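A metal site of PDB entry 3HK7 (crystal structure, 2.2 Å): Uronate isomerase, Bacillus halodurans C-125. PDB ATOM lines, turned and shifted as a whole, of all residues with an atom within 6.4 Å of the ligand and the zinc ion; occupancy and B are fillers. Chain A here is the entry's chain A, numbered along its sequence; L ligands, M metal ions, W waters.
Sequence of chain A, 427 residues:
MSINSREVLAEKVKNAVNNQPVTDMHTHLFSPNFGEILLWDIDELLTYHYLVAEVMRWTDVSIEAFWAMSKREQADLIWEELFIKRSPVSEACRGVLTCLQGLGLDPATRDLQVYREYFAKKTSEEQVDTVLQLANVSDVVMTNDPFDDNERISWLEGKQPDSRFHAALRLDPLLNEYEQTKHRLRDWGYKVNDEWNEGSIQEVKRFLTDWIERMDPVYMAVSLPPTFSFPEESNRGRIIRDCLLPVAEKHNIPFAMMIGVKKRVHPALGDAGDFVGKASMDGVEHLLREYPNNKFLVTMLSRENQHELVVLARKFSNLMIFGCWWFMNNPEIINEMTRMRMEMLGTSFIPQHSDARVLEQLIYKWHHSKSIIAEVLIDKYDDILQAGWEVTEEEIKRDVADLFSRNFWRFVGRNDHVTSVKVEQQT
Of the 21 residues printed, 3 come within 4 Å of the zinc ion.
Water W2 lies within hydrogen-bond range of an oxygen (O1) of the ligand, the side-chain hydroxyl (OG) of Ser 223 and the side-chain amino group (NZ) of Lys 263.
Water W1 lies within hydrogen-bond range of the backbone carbonyl oxygen (O) of Asp 271 (2.5 Å), the side-chain carboxylate (OD2) of Asp 274 (2.6 Å) and an oxygen (O5) of the ligand (2.7 Å).
Water W3 lies within hydrogen-bond range of the side-chain hydroxyl of Tyr 48, the backbone carbonyl oxygen of Asp 355 and an oxygen (O6) of the ligand.
Residues that only touch the ligand: Ser 223 (3.9 Å), Met 258 (3.1 Å) and Trp 326 (3.6 Å).
Hydrophobic or aromatic side chains that line the ligand: His 26, His 28, His 49, Tyr 50, Met 258, Trp 325 and Trp 326.
11 residues have an atom within 4 Å of the ligand: His 26, His 28, His 49, Tyr 50, Arg 170, Ser 223, Met 258, Trp 325, Trp 326, Asp 355 and Arg 357.
The nearest printed residue that does not touch the ligand is Asp 271 (4.2 Å).
The zinc ion is bound by O3 of the ligand (2.1 Å).
The side-chain carboxylate (OD1) of Asp 355 binds the zinc ion, at 2.1 Å.
The zinc ion is bound by NE2 of His 26, 2.2 Å away.
NE2 of His 28 binds the zinc ion (2.2 Å).
O2 of the ligand binds the zinc ion, at 2.2 Å.
OG of Ser 223 sits close to NH2 of Arg 170, at 3.2 Å.
The guanidinium group of Arg 357 lies within salt-bridge range of the side-chain carboxylate of Asp 271, 3.8 Å away.
NE2 of His 353 is in hydrogen-bond range of OD2 of Asp 355 (3.0 Å).
A ring nitrogen (ND1) of His 49 lies close to the backbone carbonyl oxygen of Asp 271, at 3.4 Å.
The side-chain carboxylate (OD2) of Asp 172 lies within hydrogen-bond range of the side-chain hydroxyl (OG) of Ser 223.
The guanidinium group of Arg 170 lies within salt-bridge range of the side-chain carboxylate of Asp 172 (2.7 Å).
OD2 of Asp 355 sits close to NE1 of Trp 325 (3.2 Å).
A ring nitrogen (NE2) of His 49 sits close to the guanidinium group (NE) of Arg 357 (3.4 Å).
A ring nitrogen (NE2) of His 49 lies within hydrogen-bond range of an oxygen (O5) of the ligand (2.8 Å).
NH2 of Arg 170 lies within salt-bridge range of O1 of the ligand, 2.7 Å away.
The side-chain hydroxyl (OH) of Tyr 50 sits at hydrogen-bond distance from an oxygen (O7) of the ligand, at 3.2 Å.
The indole nitrogen (NE1) of Trp 325 sits close to an oxygen (O3) of the ligand.
O6 of the ligand lies within salt-bridge range of NE of Arg 357 (2.9 Å).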
ATOM      1  N   HIS A  26      -2.834  18.455  22.207  1.00  0.00           N
ATOM      2  CA  HIS A  26      -3.558  19.705  21.970  1.00  0.00           C
ATOM      3  C   HIS A  26      -3.798  19.959  20.490  1.00  0.00           C
ATOM      4  O   HIS A  26      -2.857  20.220  19.730  1.00  0.00           O
ATOM      5  CB  HIS A  26      -2.855  20.936  22.561  1.00  0.00           C
ATOM      6  CG  HIS A  26      -3.594  22.220  22.289  1.00  0.00           C
ATOM      7  ND1 HIS A  26      -4.868  22.455  22.762  1.00  0.00           N
ATOM      8  CD2 HIS A  26      -3.263  23.300  21.542  1.00  0.00           C
ATOM      9  CE1 HIS A  26      -5.292  23.625  22.322  1.00  0.00           C
ATOM     10  NE2 HIS A  26      -4.335  24.167  21.579  1.00  0.00           N
ATOM     11  N   THR A  27      -5.058  19.880  20.091  1.00  0.00           N
ATOM     12  CA  THR A  27      -5.448  20.106  18.700  1.00  0.00           C
ATOM     13  C   THR A  27      -6.829  20.726  18.685  1.00  0.00           C
ATOM     14  O   THR A  27      -7.486  20.826  19.729  1.00  0.00           O
ATOM     15  CB  THR A  27      -5.547  18.793  17.884  1.00  0.00           C
ATOM     16  OG1 THR A  27      -6.742  18.091  18.266  1.00  0.00           O
ATOM     17  CG2 THR A  27      -4.347  17.896  18.149  1.00  0.00           C
ATOM     18  N   HIS A  28      -7.256  21.130  17.499  1.00  0.00           N
ATOM     19  CA  HIS A  28      -8.577  21.703  17.294  1.00  0.00           C
ATOM     20  C   HIS A  28      -9.305  20.803  16.315  1.00  0.00           C
ATOM     21  O   HIS A  28     -10.060  21.260  15.457  1.00  0.00           O
ATOM     22  CB  HIS A  28      -8.424  23.114  16.750  1.00  0.00           C
ATOM     23  CG  HIS A  28      -7.941  24.089  17.777  1.00  0.00           C
ATOM     24  ND1 HIS A  28      -8.780  24.630  18.727  1.00  0.00           N
ATOM     25  CD2 HIS A  28      -6.696  24.531  18.073  1.00  0.00           C
ATOM     26  CE1 HIS A  28      -8.064  25.367  19.564  1.00  0.00           C
ATOM     27  NE2 HIS A  28      -6.800  25.315  19.193  1.00  0.00           N
ATOM     28  N   TYR A  48      -6.357  27.926   6.194  1.00  0.00           N
ATOM     29  CA  TYR A  48      -5.937  27.882   7.601  1.00  0.00           C
ATOM     30  C   TYR A  48      -5.678  29.359   7.909  1.00  0.00           C
ATOM     31  O   TYR A  48      -5.111  30.065   7.073  1.00  0.00           O
ATOM     32  CB  TYR A  48      -4.641  27.043   7.679  1.00  0.00           C
ATOM     33  CG  TYR A  48      -3.973  26.875   9.025  1.00  0.00           C
ATOM     34  CD1 TYR A  48      -4.703  26.693  10.195  1.00  0.00           C
ATOM     35  CD2 TYR A  48      -2.581  26.798   9.107  1.00  0.00           C
ATOM     36  CE1 TYR A  48      -4.066  26.408  11.418  1.00  0.00           C
ATOM     37  CE2 TYR A  48      -1.928  26.516  10.306  1.00  0.00           C
ATOM     38  CZ  TYR A  48      -2.676  26.324  11.453  1.00  0.00           C
ATOM     39  OH  TYR A  48      -2.019  26.014  12.617  1.00  0.00           O
ATOM     40  N   HIS A  49      -6.104  29.850   9.069  1.00  0.00           N
ATOM     41  CA  HIS A  49      -5.911  31.276   9.323  1.00  0.00           C
ATOM     42  C   HIS A  49      -4.459  31.744   9.254  1.00  0.00           C
ATOM     43  O   HIS A  49      -4.190  32.909   8.962  1.00  0.00           O
ATOM     44  CB  HIS A  49      -6.609  31.709  10.620  1.00  0.00           C
ATOM     45  CG  HIS A  49      -5.907  31.326  11.889  1.00  0.00           C
ATOM     46  ND1 HIS A  49      -4.832  32.028  12.387  1.00  0.00           N
ATOM     47  CD2 HIS A  49      -6.170  30.359  12.796  1.00  0.00           C
ATOM     48  CE1 HIS A  49      -4.470  31.523  13.559  1.00  0.00           C
ATOM     49  NE2 HIS A  49      -5.269  30.517  13.830  1.00  0.00           N
ATOM     50  N   TYR A  50      -3.507  30.837   9.485  1.00  0.00           N
ATOM     51  CA  TYR A  50      -2.099  31.198   9.407  1.00  0.00           C
ATOM     52  C   TYR A  50      -1.808  31.677   7.972  1.00  0.00           C
ATOM     53  O   TYR A  50      -1.049  32.627   7.780  1.00  0.00           O
ATOM     54  CB  TYR A  50      -1.197  29.992   9.718  1.00  0.00           C
ATOM     55  CG  TYR A  50      -1.079  29.594  11.181  1.00  0.00           C
ATOM     56  CD1 TYR A  50      -2.197  29.551  12.010  1.00  0.00           C
ATOM     57  CD2 TYR A  50       0.145  29.167  11.709  1.00  0.00           C
ATOM     58  CE1 TYR A  50      -2.097  29.067  13.327  1.00  0.00           C
ATOM     59  CE2 TYR A  50       0.254  28.685  13.015  1.00  0.00           C
ATOM     60  CZ  TYR A  50      -0.872  28.641  13.820  1.00  0.00           C
ATOM     61  OH  TYR A  50      -0.769  28.144  15.102  1.00  0.00           O
ATOM     62  N   THR A 143     -10.150  20.275  21.647  1.00  0.00           N
ATOM     63  CA  THR A 143     -10.392  21.451  22.471  1.00  0.00           C
ATOM     64  C   THR A 143     -11.911  21.540  22.473  1.00  0.00           C
ATOM     65  O   THR A 143     -12.519  21.882  21.472  1.00  0.00           O
ATOM     66  CB  THR A 143      -9.813  22.726  21.830  1.00  0.00           C
ATOM     67  OG1 THR A 143      -8.385  22.599  21.704  1.00  0.00           O
ATOM     68  CG2 THR A 143     -10.136  23.948  22.687  1.00  0.00           C
ATOM     69  N   ARG A 170     -12.166  23.388  27.495  1.00  0.00           N
ATOM     70  CA  ARG A 170     -11.687  24.751  27.310  1.00  0.00           C
ATOM     71  C   ARG A 170     -12.630  25.731  28.028  1.00  0.00           C
ATOM     72  O   ARG A 170     -13.833  25.721  27.793  1.00  0.00           O
ATOM     73  CB  ARG A 170     -11.628  25.058  25.809  1.00  0.00           C
ATOM     74  CG  ARG A 170     -10.875  26.316  25.426  1.00  0.00           C
ATOM     75  CD  ARG A 170      -9.428  26.276  25.914  1.00  0.00           C
ATOM     76  NE  ARG A 170      -8.726  27.485  25.488  1.00  0.00           N
ATOM     77  CZ  ARG A 170      -8.041  27.597  24.356  1.00  0.00           C
ATOM     78  NH1 ARG A 170      -7.949  26.559  23.526  1.00  0.00           N
ATOM     79  NH2 ARG A 170      -7.487  28.750  24.036  1.00  0.00           N
ATOM     80  N   ASP A 172     -12.073  29.428  28.324  1.00  0.00           N
ATOM     81  CA  ASP A 172     -11.801  30.843  28.071  1.00  0.00           C
ATOM     82  C   ASP A 172     -12.936  31.825  28.409  1.00  0.00           C
ATOM     83  O   ASP A 172     -12.706  32.844  29.079  1.00  0.00           O
ATOM     84  CB  ASP A 172     -11.370  31.034  26.611  1.00  0.00           C
ATOM     85  CG  ASP A 172      -9.996  30.403  26.319  1.00  0.00           C
ATOM     86  OD1 ASP A 172      -9.614  29.472  27.062  1.00  0.00           O
ATOM     87  OD2 ASP A 172      -9.326  30.818  25.342  1.00  0.00           O
ATOM     88  N   SER A 223      -6.651  29.922  27.442  1.00  0.00           N
ATOM     89  CA  SER A 223      -5.569  30.712  26.862  1.00  0.00           C
ATOM     90  C   SER A 223      -5.614  32.029  27.635  1.00  0.00           C
ATOM     91  O   SER A 223      -6.682  32.564  27.903  1.00  0.00           O
ATOM     92  CB  SER A 223      -5.794  30.947  25.365  1.00  0.00           C
ATOM     93  OG  SER A 223      -6.928  31.745  25.111  1.00  0.00           O
ATOM     94  N   MET A 258      -2.299  28.294  28.626  1.00  0.00           N
ATOM     95  CA  MET A 258      -1.611  28.685  27.412  1.00  0.00           C
ATOM     96  C   MET A 258      -1.534  30.213  27.469  1.00  0.00           C
ATOM     97  O   MET A 258      -2.470  30.932  27.080  1.00  0.00           O
ATOM     98  CB  MET A 258      -2.398  28.187  26.196  1.00  0.00           C
ATOM     99  CG  MET A 258      -2.731  26.695  26.308  1.00  0.00           C
ATOM    100  SD  MET A 258      -3.004  25.891  24.722  1.00  0.00           S
ATOM    101  CE  MET A 258      -4.656  26.438  24.377  1.00  0.00           C
ATOM    102  N   VAL A 261      -1.189  35.162  24.634  1.00  0.00           N
ATOM    103  CA  VAL A 261      -1.985  35.639  23.510  1.00  0.00           C
ATOM    104  C   VAL A 261      -2.729  36.950  23.776  1.00  0.00           C
ATOM    105  O   VAL A 261      -3.395  37.099  24.792  1.00  0.00           O
ATOM    106  CB  VAL A 261      -2.993  34.545  23.035  1.00  0.00           C
ATOM    107  CG1 VAL A 261      -3.928  34.165  24.175  1.00  0.00           C
ATOM    108  CG2 VAL A 261      -3.786  35.044  21.836  1.00  0.00           C
ATOM    109  N   LYS A 263      -5.615  38.871  22.381  1.00  0.00           N
ATOM    110  CA  LYS A 263      -6.734  38.711  21.470  1.00  0.00           C
ATOM    111  C   LYS A 263      -7.201  39.931  20.695  1.00  0.00           C
ATOM    112  O   LYS A 263      -7.210  41.049  21.199  1.00  0.00           O
ATOM    113  CB  LYS A 263      -7.930  38.110  22.224  1.00  0.00           C
ATOM    114  CG  LYS A 263      -7.595  36.887  23.060  1.00  0.00           C
ATOM    115  CD  LYS A 263      -8.271  35.616  22.537  1.00  0.00           C
ATOM    116  CE  LYS A 263      -7.691  35.175  21.197  1.00  0.00           C
ATOM    117  NZ  LYS A 263      -8.247  33.862  20.740  1.00  0.00           N
ATOM    118  N   ASP A 271      -9.853  34.866  13.277  1.00  0.00           N
ATOM    119  CA  ASP A 271      -8.929  33.985  13.993  1.00  0.00           C
ATOM    120  C   ASP A 271      -7.469  34.334  13.748  1.00  0.00           C
ATOM    121  O   ASP A 271      -6.599  33.951  14.523  1.00  0.00           O
ATOM    122  CB  ASP A 271      -9.166  32.519  13.604  1.00  0.00           C
ATOM    123  CG  ASP A 271     -10.489  31.991  14.079  1.00  0.00           C
ATOM    124  OD1 ASP A 271     -10.972  32.470  15.134  1.00  0.00           O
ATOM    125  OD2 ASP A 271     -11.048  31.087  13.427  1.00  0.00           O
ATOM    126  N   ALA A 272      -7.203  35.061  12.675  1.00  0.00           N
ATOM    127  CA  ALA A 272      -5.843  35.463  12.337  1.00  0.00           C
ATOM    128  C   ALA A 272      -5.465  36.830  12.923  1.00  0.00           C
ATOM    129  O   ALA A 272      -4.407  37.371  12.598  1.00  0.00           O
ATOM    130  CB  ALA A 272      -5.700  35.511  10.816  1.00  0.00           C
ATOM    131  N   ASP A 274      -4.910  37.660  16.289  1.00  0.00           N
ATOM    132  CA  ASP A 274      -4.366  37.654  17.641  1.00  0.00           C
ATOM    133  C   ASP A 274      -2.855  37.949  17.622  1.00  0.00           C
ATOM    134  O   ASP A 274      -2.157  37.532  16.706  1.00  0.00           O
ATOM    135  CB  ASP A 274      -4.608  36.307  18.328  1.00  0.00           C
ATOM    136  CG  ASP A 274      -6.079  36.042  18.574  1.00  0.00           C
ATOM    137  OD1 ASP A 274      -6.816  37.005  18.886  1.00  0.00           O
ATOM    138  OD2 ASP A 274      -6.497  34.870  18.463  1.00  0.00           O
ATOM    139  N   TRP A 325       4.095  26.423  20.893  1.00  0.00           N
ATOM    140  CA  TRP A 325       2.820  26.991  20.528  1.00  0.00           C
ATOM    141  C   TRP A 325       2.728  28.148  19.547  1.00  0.00           C
ATOM    142  O   TRP A 325       3.448  29.145  19.667  1.00  0.00           O
ATOM    143  CB  TRP A 325       2.102  27.393  21.824  1.00  0.00           C
ATOM    144  CG  TRP A 325       0.689  27.875  21.691  1.00  0.00           C
ATOM    145  CD1 TRP A 325      -0.266  27.392  20.847  1.00  0.00           C
ATOM    146  CD2 TRP A 325       0.039  28.863  22.503  1.00  0.00           C
ATOM    147  NE1 TRP A 325      -1.471  28.003  21.085  1.00  0.00           N
ATOM    148  CE2 TRP A 325      -1.313  28.914  22.104  1.00  0.00           C
ATOM    149  CE3 TRP A 325       0.468  29.709  23.538  1.00  0.00           C
ATOM    150  CZ2 TRP A 325      -2.246  29.783  22.693  1.00  0.00           C
ATOM    151  CZ3 TRP A 325      -0.452  30.573  24.127  1.00  0.00           C
ATOM    152  CH2 TRP A 325      -1.797  30.604  23.704  1.00  0.00           C
ATOM    153  N   TRP A 326       1.860  27.979  18.554  1.00  0.00           N
ATOM    154  CA  TRP A 326       1.541  29.035  17.589  1.00  0.00           C
ATOM    155  C   TRP A 326       2.721  29.746  16.941  1.00  0.00           C
ATOM    156  O   TRP A 326       3.377  29.209  16.051  1.00  0.00           O
ATOM    157  CB  TRP A 326       0.688  30.047  18.350  1.00  0.00           C
ATOM    158  CG  TRP A 326      -0.333  30.825  17.596  1.00  0.00           C
ATOM    159  CD1 TRP A 326      -0.286  31.220  16.298  1.00  0.00           C
ATOM    160  CD2 TRP A 326      -1.490  31.451  18.170  1.00  0.00           C
ATOM    161  NE1 TRP A 326      -1.343  32.057  16.017  1.00  0.00           N
ATOM    162  CE2 TRP A 326      -2.099  32.214  17.153  1.00  0.00           C
ATOM    163  CE3 TRP A 326      -2.070  31.429  19.450  1.00  0.00           C
ATOM    164  CZ2 TRP A 326      -3.260  32.966  17.376  1.00  0.00           C
ATOM    165  CZ3 TRP A 326      -3.218  32.175  19.674  1.00  0.00           C
ATOM    166  CH2 TRP A 326      -3.801  32.928  18.640  1.00  0.00           C
ATOM    167  N   HIS A 353       3.098  19.637  20.217  1.00  0.00           N
ATOM    168  CA  HIS A 353       1.679  19.385  19.973  1.00  0.00           C
ATOM    169  C   HIS A 353       1.433  20.050  18.604  1.00  0.00           C
ATOM    170  O   HIS A 353       2.145  20.989  18.244  1.00  0.00           O
ATOM    171  CB  HIS A 353       0.788  19.988  21.067  1.00  0.00           C
ATOM    172  CG  HIS A 353       0.699  21.482  21.033  1.00  0.00           C
ATOM    173  ND1 HIS A 353       1.564  22.297  21.742  1.00  0.00           N
ATOM    174  CD2 HIS A 353      -0.180  22.311  20.415  1.00  0.00           C
ATOM    175  CE1 HIS A 353       1.229  23.561  21.554  1.00  0.00           C
ATOM    176  NE2 HIS A 353       0.182  23.594  20.751  1.00  0.00           N
ATOM    177  N   ASP A 355      -1.645  21.460  17.330  1.00  0.00           N
ATOM    178  CA  ASP A 355      -2.569  22.588  17.328  1.00  0.00           C
ATOM    179  C   ASP A 355      -3.335  22.558  15.994  1.00  0.00           C
ATOM    180  O   ASP A 355      -3.794  23.589  15.505  1.00  0.00           O
ATOM    181  CB  ASP A 355      -1.807  23.904  17.443  1.00  0.00           C
ATOM    182  CG  ASP A 355      -2.414  24.838  18.457  1.00  0.00           C
ATOM    183  OD1 ASP A 355      -3.649  25.035  18.432  1.00  0.00           O
ATOM    184  OD2 ASP A 355      -1.664  25.379  19.297  1.00  0.00           O
ATOM    185  N   ARG A 357      -5.965  22.507  13.179  1.00  0.00           N
ATOM    186  CA  ARG A 357      -7.324  22.990  13.007  1.00  0.00           C
ATOM    187  C   ARG A 357      -7.926  22.201  11.842  1.00  0.00           C
ATOM    188  O   ARG A 357      -9.138  21.995  11.783  1.00  0.00           O
ATOM    189  CB  ARG A 357      -7.344  24.490  12.663  1.00  0.00           C
ATOM    190  CG  ARG A 357      -7.331  25.430  13.869  1.00  0.00           C
ATOM    191  CD  ARG A 357      -7.247  26.880  13.393  1.00  0.00           C
ATOM    192  NE  ARG A 357      -7.278  27.838  14.489  1.00  0.00           N
ATOM    193  CZ  ARG A 357      -8.387  28.270  15.096  1.00  0.00           C
ATOM    194  NH1 ARG A 357      -9.574  27.815  14.709  1.00  0.00           N
ATOM    195  NH2 ARG A 357      -8.310  29.150  16.077  1.00  0.00           N
HETATM  196  O1  LIG L   1      -6.050  29.360  21.855  1.00  0.00           O
HETATM  197  C1  LIG L   1      -5.571  28.390  21.202  1.00  0.00           C
HETATM  198  O2  LIG L   1      -5.700  27.192  21.514  1.00  0.00           O
HETATM  199  C2  LIG L   1      -4.758  28.713  19.932  1.00  0.00           C
HETATM  200  O3  LIG L   1      -3.979  27.557  19.595  1.00  0.00           O
HETATM  201  C3  LIG L   1      -5.659  29.099  18.729  1.00  0.00           C
HETATM  202  O4  LIG L   1      -6.415  27.952  18.311  1.00  0.00           O
HETATM  203  C4  LIG L   1      -4.857  29.655  17.503  1.00  0.00           C
HETATM  204  O5  LIG L   1      -5.712  30.384  16.619  1.00  0.00           O
HETATM  205  C5  LIG L   1      -4.147  28.554  16.663  1.00  0.00           C
HETATM  206  O6  LIG L   1      -4.611  28.282  15.533  1.00  0.00           O
HETATM  207  O7  LIG L   1      -3.137  28.000  17.178  1.00  0.00           O
HETATM  208 ZN    ZN M   1      -4.811  25.709  20.093  1.00  0.00          ZN
HETATM  209  O   HOH W   1      -6.704  32.899  16.790  1.00  0.00           O
HETATM  210  O   HOH W   2      -6.663  31.856  22.295  1.00  0.00           O
HETATM  211  O   HOH W   3      -3.669  25.945  14.480  1.00  0.00           O
